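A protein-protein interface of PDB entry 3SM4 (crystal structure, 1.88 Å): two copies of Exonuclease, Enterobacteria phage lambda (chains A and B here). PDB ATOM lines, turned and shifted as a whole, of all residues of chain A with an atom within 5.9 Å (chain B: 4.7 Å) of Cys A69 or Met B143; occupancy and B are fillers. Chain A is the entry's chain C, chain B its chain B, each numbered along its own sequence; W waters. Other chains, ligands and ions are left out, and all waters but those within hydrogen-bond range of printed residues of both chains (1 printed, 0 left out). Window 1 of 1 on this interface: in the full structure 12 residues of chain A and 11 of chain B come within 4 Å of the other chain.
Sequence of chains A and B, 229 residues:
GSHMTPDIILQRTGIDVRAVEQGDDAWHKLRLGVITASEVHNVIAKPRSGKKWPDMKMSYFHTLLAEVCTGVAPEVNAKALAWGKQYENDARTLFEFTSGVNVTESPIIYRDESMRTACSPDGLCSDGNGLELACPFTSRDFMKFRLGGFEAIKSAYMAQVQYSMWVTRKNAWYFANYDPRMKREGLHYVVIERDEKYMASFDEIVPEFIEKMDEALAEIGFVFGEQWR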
ATOM      1  N   PHE A  61     -15.975  -8.392   2.387  1.00  0.00           N
ATOM      2  CA  PHE A  61     -14.979  -8.892   1.441  1.00  0.00           C
ATOM      3  C   PHE A  61     -13.573  -8.452   1.855  1.00  0.00           C
ATOM      4  O   PHE A  61     -12.672  -9.283   1.980  1.00  0.00           O
ATOM      5  CB  PHE A  61     -15.327  -8.401   0.027  1.00  0.00           C
ATOM      6  CG  PHE A  61     -14.360  -8.830  -1.041  1.00  0.00           C
ATOM      7  CD1 PHE A  61     -14.277 -10.159  -1.439  1.00  0.00           C
ATOM      8  CD2 PHE A  61     -13.562  -7.888  -1.681  1.00  0.00           C
ATOM      9  CE1 PHE A  61     -13.392 -10.548  -2.442  1.00  0.00           C
ATOM     10  CE2 PHE A  61     -12.678  -8.264  -2.688  1.00  0.00           C
ATOM     11  CZ  PHE A  61     -12.589  -9.598  -3.068  1.00  0.00           C
ATOM     12  N   HIS A  62     -13.402  -7.154   2.105  1.00  0.00           N
ATOM     13  CA  HIS A  62     -12.114  -6.616   2.558  1.00  0.00           C
ATOM     14  C   HIS A  62     -11.752  -7.050   3.979  1.00  0.00           C
ATOM     15  O   HIS A  62     -10.578  -7.222   4.291  1.00  0.00           O
ATOM     16  CB  HIS A  62     -12.085  -5.085   2.452  1.00  0.00           C
ATOM     17  CG  HIS A  62     -12.206  -4.571   1.051  1.00  0.00           C
ATOM     18  ND1 HIS A  62     -13.183  -3.679   0.667  1.00  0.00           N
ATOM     19  CD2 HIS A  62     -11.474  -4.827  -0.060  1.00  0.00           C
ATOM     20  CE1 HIS A  62     -13.045  -3.404  -0.618  1.00  0.00           C
ATOM     21  NE2 HIS A  62     -12.018  -4.092  -1.083  1.00  0.00           N
ATOM     22  N   LEU A  64     -12.514  -9.977   5.518  1.00  0.00           N
ATOM     23  CA  LEU A  64     -12.038 -11.355   5.502  1.00  0.00           C
ATOM     24  C   LEU A  64     -10.652 -11.476   4.866  1.00  0.00           C
ATOM     25  O   LEU A  64      -9.798 -12.195   5.383  1.00  0.00           O
ATOM     26  CB  LEU A  64     -13.044 -12.276   4.810  1.00  0.00           C
ATOM     27  CG  LEU A  64     -14.295 -12.727   5.571  1.00  0.00           C
ATOM     28  CD1 LEU A  64     -15.041 -13.772   4.753  1.00  0.00           C
ATOM     29  CD2 LEU A  64     -13.956 -13.281   6.953  1.00  0.00           C
ATOM     30  N   LEU A  65     -10.428 -10.767   3.760  1.00  0.00           N
ATOM     31  CA  LEU A  65      -9.114 -10.736   3.103  1.00  0.00           C
ATOM     32  C   LEU A  65      -8.026 -10.225   4.054  1.00  0.00           C
ATOM     33  O   LEU A  65      -6.901 -10.732   4.050  1.00  0.00           O
ATOM     34  CB  LEU A  65      -9.146  -9.856   1.847  1.00  0.00           C
ATOM     35  CG  LEU A  65      -9.905 -10.308   0.593  1.00  0.00           C
ATOM     36  CD1 LEU A  65     -10.021  -9.156  -0.386  1.00  0.00           C
ATOM     37  CD2 LEU A  65      -9.238 -11.499  -0.076  1.00  0.00           C
ATOM     38  N   ALA A  66      -8.380  -9.224   4.858  1.00  0.00           N
ATOM     39  CA  ALA A  66      -7.483  -8.649   5.861  1.00  0.00           C
ATOM     40  C   ALA A  66      -7.111  -9.653   6.952  1.00  0.00           C
ATOM     41  O   ALA A  66      -5.975  -9.658   7.434  1.00  0.00           O
ATOM     42  CB  ALA A  66      -8.104  -7.389   6.473  1.00  0.00           C
ATOM     43  N   GLU A  67      -8.063 -10.504   7.333  1.00  0.00           N
ATOM     44  CA  GLU A  67      -7.811 -11.570   8.306  1.00  0.00           C
ATOM     45  C   GLU A  67      -6.809 -12.593   7.774  1.00  0.00           C
ATOM     46  O   GLU A  67      -5.975 -13.097   8.525  1.00  0.00           O
ATOM     47  CB  GLU A  67      -9.116 -12.270   8.713  1.00  0.00           C
ATOM     48  CG  GLU A  67     -10.024 -11.411   9.588  1.00  0.00           C
ATOM     49  CD  GLU A  67     -11.363 -12.060   9.902  1.00  0.00           C
ATOM     50  OE1 GLU A  67     -11.493 -13.301   9.786  1.00  0.00           O
ATOM     51  OE2 GLU A  67     -12.294 -11.317  10.287  1.00  0.00           O
ATOM     52  N   VAL A  68      -6.899 -12.893   6.480  1.00  0.00           N
ATOM     53  CA  VAL A  68      -5.981 -13.839   5.833  1.00  0.00           C
ATOM     54  C   VAL A  68      -4.554 -13.276   5.792  1.00  0.00           C
ATOM     55  O   VAL A  68      -3.579 -13.993   6.049  1.00  0.00           O
ATOM     56  CB  VAL A  68      -6.460 -14.218   4.404  1.00  0.00           C
ATOM     57  CG1 VAL A  68      -5.425 -15.077   3.678  1.00  0.00           C
ATOM     58  CG2 VAL A  68      -7.806 -14.943   4.456  1.00  0.00           C
ATOM     59  N   CYS A  69      -4.443 -11.987   5.487  1.00  0.00           N
ATOM     60  CA  CYS A  69      -3.141 -11.358   5.280  1.00  0.00           C
ATOM     61  C   CYS A  69      -2.455 -10.881   6.566  1.00  0.00           C
ATOM     62  O   CYS A  69      -1.231 -10.736   6.598  1.00  0.00           O
ATOM     63  CB  CYS A  69      -3.257 -10.229   4.255  1.00  0.00           C
ATOM     64  SG  CYS A  69      -3.790 -10.788   2.612  1.00  0.00           S
ATOM     65  N   THR A  70      -3.235 -10.639   7.621  1.00  0.00           N
ATOM     66  CA  THR A  70      -2.668 -10.248   8.915  1.00  0.00           C
ATOM     67  C   THR A  70      -2.579 -11.420   9.893  1.00  0.00           C
ATOM     68  O   THR A  70      -1.765 -11.401  10.817  1.00  0.00           O
ATOM     69  CB  THR A  70      -3.455  -9.094   9.593  1.00  0.00           C
ATOM     70  OG1 THR A  70      -4.807  -9.501   9.826  1.00  0.00           O
ATOM     71  CG2 THR A  70      -3.440  -7.825   8.741  1.00  0.00           C
ATOM     72  N   GLY A  71      -3.427 -12.428   9.695  1.00  0.00           N
ATOM     73  CA  GLY A  71      -3.529 -13.544  10.629  1.00  0.00           C
ATOM     74  C   GLY A  71      -4.171 -13.162  11.954  1.00  0.00           C
ATOM     75  O   GLY A  71      -4.118 -13.932  12.913  1.00  0.00           O
ATOM     76  N   LEU A 217      -6.606 -12.232  -3.284  1.00  0.00           N
ATOM     77  CA  LEU A 217      -5.438 -12.765  -2.576  1.00  0.00           C
ATOM     78  C   LEU A 217      -4.266 -13.008  -3.529  1.00  0.00           C
ATOM     79  O   LEU A 217      -3.122 -12.660  -3.218  1.00  0.00           O
ATOM     80  CB  LEU A 217      -5.795 -14.052  -1.818  1.00  0.00           C
ATOM     81  CG  LEU A 217      -6.688 -13.940  -0.575  1.00  0.00           C
ATOM     82  CD1 LEU A 217      -7.234 -15.303  -0.167  1.00  0.00           C
ATOM     83  CD2 LEU A 217      -5.960 -13.278   0.588  1.00  0.00           C
ATOM     84  N   ILE A 220      -2.308  -9.893  -4.698  1.00  0.00           N
ATOM     85  CA  ILE A 220      -1.332  -9.346  -3.745  1.00  0.00           C
ATOM     86  C   ILE A 220      -0.348 -10.400  -3.202  1.00  0.00           C
ATOM     87  O   ILE A 220       0.358 -10.154  -2.219  1.00  0.00           O
ATOM     88  CB  ILE A 220      -2.016  -8.570  -2.582  1.00  0.00           C
ATOM     89  CG1 ILE A 220      -3.028  -9.460  -1.849  1.00  0.00           C
ATOM     90  CG2 ILE A 220      -2.666  -7.291  -3.108  1.00  0.00           C
ATOM     91  CD1 ILE A 220      -3.445  -8.939  -0.491  1.00  0.00           C
ATOM     92  N   PHE A 222      -0.884 -13.569  -1.915  1.00  0.00           N
ATOM     93  CA  PHE A 222      -1.293 -14.343  -0.748  1.00  0.00           C
ATOM     94  C   PHE A 222      -2.135 -15.546  -1.154  1.00  0.00           C
ATOM     95  O   PHE A 222      -2.750 -15.552  -2.224  1.00  0.00           O
ATOM     96  CB  PHE A 222      -2.090 -13.469   0.230  1.00  0.00           C
ATOM     97  CG  PHE A 222      -1.236 -12.715   1.210  1.00  0.00           C
ATOM     98  CD1 PHE A 222      -0.743 -11.450   0.896  1.00  0.00           C
ATOM     99  CD2 PHE A 222      -0.935 -13.262   2.453  1.00  0.00           C
ATOM    100  CE1 PHE A 222       0.042 -10.745   1.805  1.00  0.00           C
ATOM    101  CE2 PHE A 222      -0.150 -12.567   3.367  1.00  0.00           C
ATOM    102  CZ  PHE A 222       0.340 -11.304   3.043  1.00  0.00           C
ATOM    103  N   GLN A 227      -2.996 -17.662   7.209  1.00  0.00           N
ATOM    104  CA  GLN A 227      -3.385 -17.186   8.537  1.00  0.00           C
ATOM    105  C   GLN A 227      -3.147 -18.237   9.623  1.00  0.00           C
ATOM    106  O   GLN A 227      -2.990 -17.898  10.797  1.00  0.00           O
ATOM    107  CB  GLN A 227      -4.855 -16.734   8.549  1.00  0.00           C
ATOM    108  CG  GLN A 227      -5.892 -17.847   8.348  1.00  0.00           C
ATOM    109  CD  GLN A 227      -6.265 -18.077   6.887  1.00  0.00           C
ATOM    110  OE1 GLN A 227      -5.454 -17.890   5.981  1.00  0.00           O
ATOM    111  NE2 GLN A 227      -7.505 -18.484   6.659  1.00  0.00           N
ATOM    112  N   SER B 139      -7.688  -3.121   9.381  1.00  0.00           N
ATOM    113  CA  SER B 139      -6.952  -3.718   8.271  1.00  0.00           C
ATOM    114  C   SER B 139      -7.843  -3.819   7.032  1.00  0.00           C
ATOM    115  O   SER B 139      -7.348  -3.817   5.903  1.00  0.00           O
ATOM    116  CB  SER B 139      -6.389  -5.083   8.667  1.00  0.00           C
ATOM    117  OG  SER B 139      -5.397  -4.952   9.677  1.00  0.00           O
ATOM    118  N   ARG B 140      -9.153  -3.885   7.265  1.00  0.00           N
ATOM    119  CA  ARG B 140     -10.172  -3.811   6.215  1.00  0.00           C
ATOM    120  C   ARG B 140      -9.949  -2.609   5.298  1.00  0.00           C
ATOM    121  O   ARG B 140      -9.872  -2.756   4.074  1.00  0.00           O
ATOM    122  CB  ARG B 140     -11.570  -3.735   6.850  1.00  0.00           C
ATOM    123  CG  ARG B 140     -12.714  -3.458   5.873  1.00  0.00           C
ATOM    124  CD  ARG B 140     -13.951  -2.939   6.601  1.00  0.00           C
ATOM    125  NE  ARG B 140     -13.760  -1.577   7.097  1.00  0.00           N
ATOM    126  CZ  ARG B 140     -14.389  -1.052   8.147  1.00  0.00           C
ATOM    127  NH1 ARG B 140     -15.263  -1.768   8.846  1.00  0.00           N
ATOM    128  NH2 ARG B 140     -14.136   0.200   8.501  1.00  0.00           N
ATOM    129  N   ASP B 141      -9.846  -1.425   5.900  1.00  0.00           N
ATOM    130  CA  ASP B 141      -9.708  -0.184   5.146  1.00  0.00           C
ATOM    131  C   ASP B 141      -8.343  -0.043   4.479  1.00  0.00           C
ATOM    132  O   ASP B 141      -8.246   0.530   3.391  1.00  0.00           O
ATOM    133  CB  ASP B 141     -10.037   1.031   6.022  1.00  0.00           C
ATOM    134  CG  ASP B 141     -11.534   1.194   6.256  1.00  0.00           C
ATOM    135  OD1 ASP B 141     -12.325   0.396   5.705  1.00  0.00           O
ATOM    136  OD2 ASP B 141     -11.923   2.118   6.999  1.00  0.00           O
ATOM    137  N   PHE B 142      -7.299  -0.577   5.113  1.00  0.00           N
ATOM    138  CA  PHE B 142      -6.000  -0.682   4.453  1.00  0.00           C
ATOM    139  C   PHE B 142      -6.104  -1.573   3.214  1.00  0.00           C
ATOM    140  O   PHE B 142      -5.560  -1.237   2.159  1.00  0.00           O
ATOM    141  CB  PHE B 142      -4.903  -1.213   5.390  1.00  0.00           C
ATOM    142  CG  PHE B 142      -3.606  -1.517   4.679  1.00  0.00           C
ATOM    143  CD1 PHE B 142      -3.349  -2.794   4.185  1.00  0.00           C
ATOM    144  CD2 PHE B 142      -2.659  -0.519   4.472  1.00  0.00           C
ATOM    145  CE1 PHE B 142      -2.165  -3.075   3.511  1.00  0.00           C
ATOM    146  CE2 PHE B 142      -1.470  -0.790   3.799  1.00  0.00           C
ATOM    147  CZ  PHE B 142      -1.223  -2.068   3.318  1.00  0.00           C
ATOM    148  N   MET B 143      -6.798  -2.703   3.352  1.00  0.00           N
ATOM    149  CA  MET B 143      -6.990  -3.644   2.250  1.00  0.00           C
ATOM    150  C   MET B 143      -7.770  -3.012   1.094  1.00  0.00           C
ATOM    151  O   MET B 143      -7.481  -3.287  -0.073  1.00  0.00           O
ATOM    152  CB  MET B 143      -7.679  -4.925   2.740  1.00  0.00           C
ATOM    153  CG  MET B 143      -7.835  -6.027   1.695  1.00  0.00           C
ATOM    154  SD  MET B 143      -6.286  -6.607   0.963  1.00  0.00           S
ATOM    155  CE  MET B 143      -5.441  -7.240   2.412  1.00  0.00           C
ATOM    156  N   LYS B 144      -8.743  -2.164   1.426  1.00  0.00           N
ATOM    157  CA  LYS B 144      -9.522  -1.431   0.427  1.00  0.00           C
ATOM    158  C   LYS B 144      -8.630  -0.514  -0.418  1.00  0.00           C
ATOM    159  O   LYS B 144      -8.808  -0.422  -1.634  1.00  0.00           O
ATOM    160  CB  LYS B 144     -10.638  -0.624   1.098  1.00  0.00           C
ATOM    161  CG  LYS B 144     -11.589   0.067   0.124  1.00  0.00           C
ATOM    162  CD  LYS B 144     -12.618   0.910   0.858  1.00  0.00           C
ATOM    163  CE  LYS B 144     -13.476   1.703  -0.122  1.00  0.00           C
ATOM    164  NZ  LYS B 144     -14.601   2.406   0.559  1.00  0.00           N
ATOM    165  N   PHE B 145      -7.677   0.153   0.231  1.00  0.00           N
ATOM    166  CA  PHE B 145      -6.722   1.019  -0.467  1.00  0.00           C
ATOM    167  C   PHE B 145      -5.673   0.216  -1.233  1.00  0.00           C
ATOM    168  O   PHE B 145      -5.340   0.552  -2.373  1.00  0.00           O
ATOM    169  CB  PHE B 145      -6.053   2.005   0.501  1.00  0.00           C
ATOM    170  CG  PHE B 145      -5.046   2.914  -0.157  1.00  0.00           C
ATOM    171  CD1 PHE B 145      -5.446   3.858  -1.096  1.00  0.00           C
ATOM    172  CD2 PHE B 145      -3.694   2.818   0.158  1.00  0.00           C
ATOM    173  CE1 PHE B 145      -4.511   4.692  -1.716  1.00  0.00           C
ATOM    174  CE2 PHE B 145      -2.754   3.652  -0.448  1.00  0.00           C
ATOM    175  CZ  PHE B 145      -3.163   4.586  -1.385  1.00  0.00           C
ATOM    176  N   ARG B 146      -5.160  -0.843  -0.608  1.00  0.00           N
ATOM    177  CA  ARG B 146      -4.192  -1.734  -1.261  1.00  0.00           C
ATOM    178  C   ARG B 146      -4.721  -2.289  -2.591  1.00  0.00           C
ATOM    179  O   ARG B 146      -3.980  -2.370  -3.573  1.00  0.00           O
ATOM    180  CB  ARG B 146      -3.783  -2.880  -0.321  1.00  0.00           C
ATOM    181  CG  ARG B 146      -2.768  -3.878  -0.908  1.00  0.00           C
ATOM    182  CD  ARG B 146      -1.404  -3.237  -1.166  1.00  0.00           C
ATOM    183  NE  ARG B 146      -0.497  -4.113  -1.917  1.00  0.00           N
ATOM    184  CZ  ARG B 146      -0.465  -4.214  -3.245  1.00  0.00           C
ATOM    185  NH1 ARG B 146      -1.296  -3.505  -3.995  1.00  0.00           N
ATOM    186  NH2 ARG B 146       0.400  -5.036  -3.829  1.00  0.00           N
ATOM    187  N   LEU B 147      -6.004  -2.642  -2.619  1.00  0.00           N
ATOM    188  CA  LEU B 147      -6.610  -3.263  -3.801  1.00  0.00           C
ATOM    189  C   LEU B 147      -7.180  -2.268  -4.812  1.00  0.00           C
ATOM    190  O   LEU B 147      -7.126  -2.507  -6.018  1.00  0.00           O
ATOM    191  CB  LEU B 147      -7.693  -4.268  -3.391  1.00  0.00           C
ATOM    192  CG  LEU B 147      -7.271  -5.519  -2.612  1.00  0.00           C
ATOM    193  CD1 LEU B 147      -8.501  -6.221  -2.072  1.00  0.00           C
ATOM    194  CD2 LEU B 147      -6.431  -6.476  -3.463  1.00  0.00           C
ATOM    195  N   ARG B 181       0.343  -4.779  10.965  1.00  0.00           N
ATOM    196  CA  ARG B 181      -0.197  -6.129  11.162  1.00  0.00           C
ATOM    197  C   ARG B 181      -0.053  -7.023   9.931  1.00  0.00           C
ATOM    198  O   ARG B 181      -0.046  -8.248  10.048  1.00  0.00           O
ATOM    199  CB  ARG B 181      -1.670  -6.067  11.576  1.00  0.00           C
ATOM    200  CG  ARG B 181      -1.911  -5.508  12.969  1.00  0.00           C
ATOM    201  CD  ARG B 181      -3.320  -4.940  13.099  1.00  0.00           C
ATOM    202  NE  ARG B 181      -3.533  -3.786  12.222  1.00  0.00           N
ATOM    203  CZ  ARG B 181      -4.546  -2.928  12.335  1.00  0.00           C
ATOM    204  NH1 ARG B 181      -5.446  -3.073  13.300  1.00  0.00           N
ATOM    205  NH2 ARG B 181      -4.653  -1.912  11.490  1.00  0.00           N
ATOM    206  N   MET B 182       0.041  -6.409   8.754  1.00  0.00           N
ATOM    207  CA  MET B 182       0.209  -7.152   7.506  1.00  0.00           C
ATOM    208  C   MET B 182       1.541  -7.898   7.497  1.00  0.00           C
ATOM    209  O   MET B 182       2.600  -7.288   7.675  1.00  0.00           O
ATOM    210  CB  MET B 182       0.121  -6.207   6.305  1.00  0.00           C
ATOM    211  CG  MET B 182      -1.272  -5.640   6.042  1.00  0.00           C
ATOM    212  SD  MET B 182      -2.392  -6.813   5.250  1.00  0.00           S
ATOM    213  CE  MET B 182      -1.784  -6.782   3.564  1.00  0.00           C
ATOM    214  N   LYS B 183       1.483  -9.214   7.301  1.00  0.00           N
ATOM    215  CA  LYS B 183       2.695 -10.034   7.216  1.00  0.00           C
ATOM    216  C   LYS B 183       3.587  -9.540   6.076  1.00  0.00           C
ATOM    217  O   LYS B 183       4.782  -9.320   6.269  1.00  0.00           O
ATOM    218  CB  LYS B 183       2.351 -11.520   7.062  1.00  0.00           C
ATOM    219  CG  LYS B 183       2.096 -12.237   8.395  1.00  0.00           C
ATOM    220  CD  LYS B 183       1.616 -13.678   8.217  1.00  0.00           C
ATOM    221  CE  LYS B 183       2.719 -14.619   7.739  1.00  0.00           C
ATOM    222  NZ  LYS B 183       2.237 -16.027   7.622  1.00  0.00           N
HETATM  223  O   HOH W   1      -0.271  -9.460  12.247  1.00  0.00           O
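N of Lys B183 sits at hydrogen-bond distance from O of Cys A69 (3.2 Å).
The backbone carbonyl oxygen of Ala A66 is in hydrogen-bond range of the side-chain hydroxyl of Thr A70 (2.7 Å). OD1 of Asp B141 is in salt-bridge range of NE of Arg B140 (2.8 Å). The backbone carbonyl oxygen of Leu A65 lies within hydrogen-bond range of the side-chain sulfur of Cys A69, 3.4 Å away. The side-chain hydroxyl (OG) of Ser B139 sits at hydrogen-bond distance from the guanidinium group (NE) of Arg B181 (3.4 Å).
His A62 touches Arg B140 (CB to O, 3.6 Å). Met B143 touches His A62 (CG to O, 3.96 Å). His A62 touches Lys B144 (CE1 to CG, 3.8 Å). CD1 of Leu B147 touches CD1 of Leu A65, 3.7 Å away. Ala A66 touches Arg B140. Met B182 touches Cys A69. Arg B181 touches Thr A70. N of Met B182 touches CG2 of Thr A70 (3.8 Å). Ile A220 touches Met B143. Arg B146 touches Ile A220.
Met B143 touches just these residues of chain A: His A62 (3.96 Å), Cys A69 (3.9 Å) and Ile A220 (3.9 Å). Of the printed residues of chain B, Ala A66 touches Ser B139 and Arg B140. Of the printed residues of chain A, Leu B147 touches His A62 (3.9 Å), Leu A65 (3.7 Å) and Ile A220 (3.9 Å). Of the printed residues of chain B, Thr A70 touches Ser B139 (3.6 Å), Arg B181 (3.5 Å) and Met B182 (3.8 Å). Of the printed residues of chain A, Met B182 touches Cys A69 and Thr A70. Val A68 touches none of the printed residues of chain B. Leu A64 touches none of the printed residues of chain B. The nearest residue of chain A that does not touch Met B143 is Leu A65 (4.1 Å). The nearest printed residue of chain B that does not touch Ala A66 is Met B143 (4.2 Å).
Of the 14 printed residues of chain A, 6 touch a printed residue of chain B. Among the printed residues, 16 pairs touch across the chains. Among the printed residues, no Asp or Glu carboxylate lies within 4 Å of a Lys or Arg side-chain nitrogen of the other chain.
No position is printed for both chains.
Water W1 lies within hydrogen-bond range of the backbone carbonyl oxygen (O) of Arg B181 (2.5 Å) and the backbone carbonyl oxygen (O) of Thr A70 (2.8 Å).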
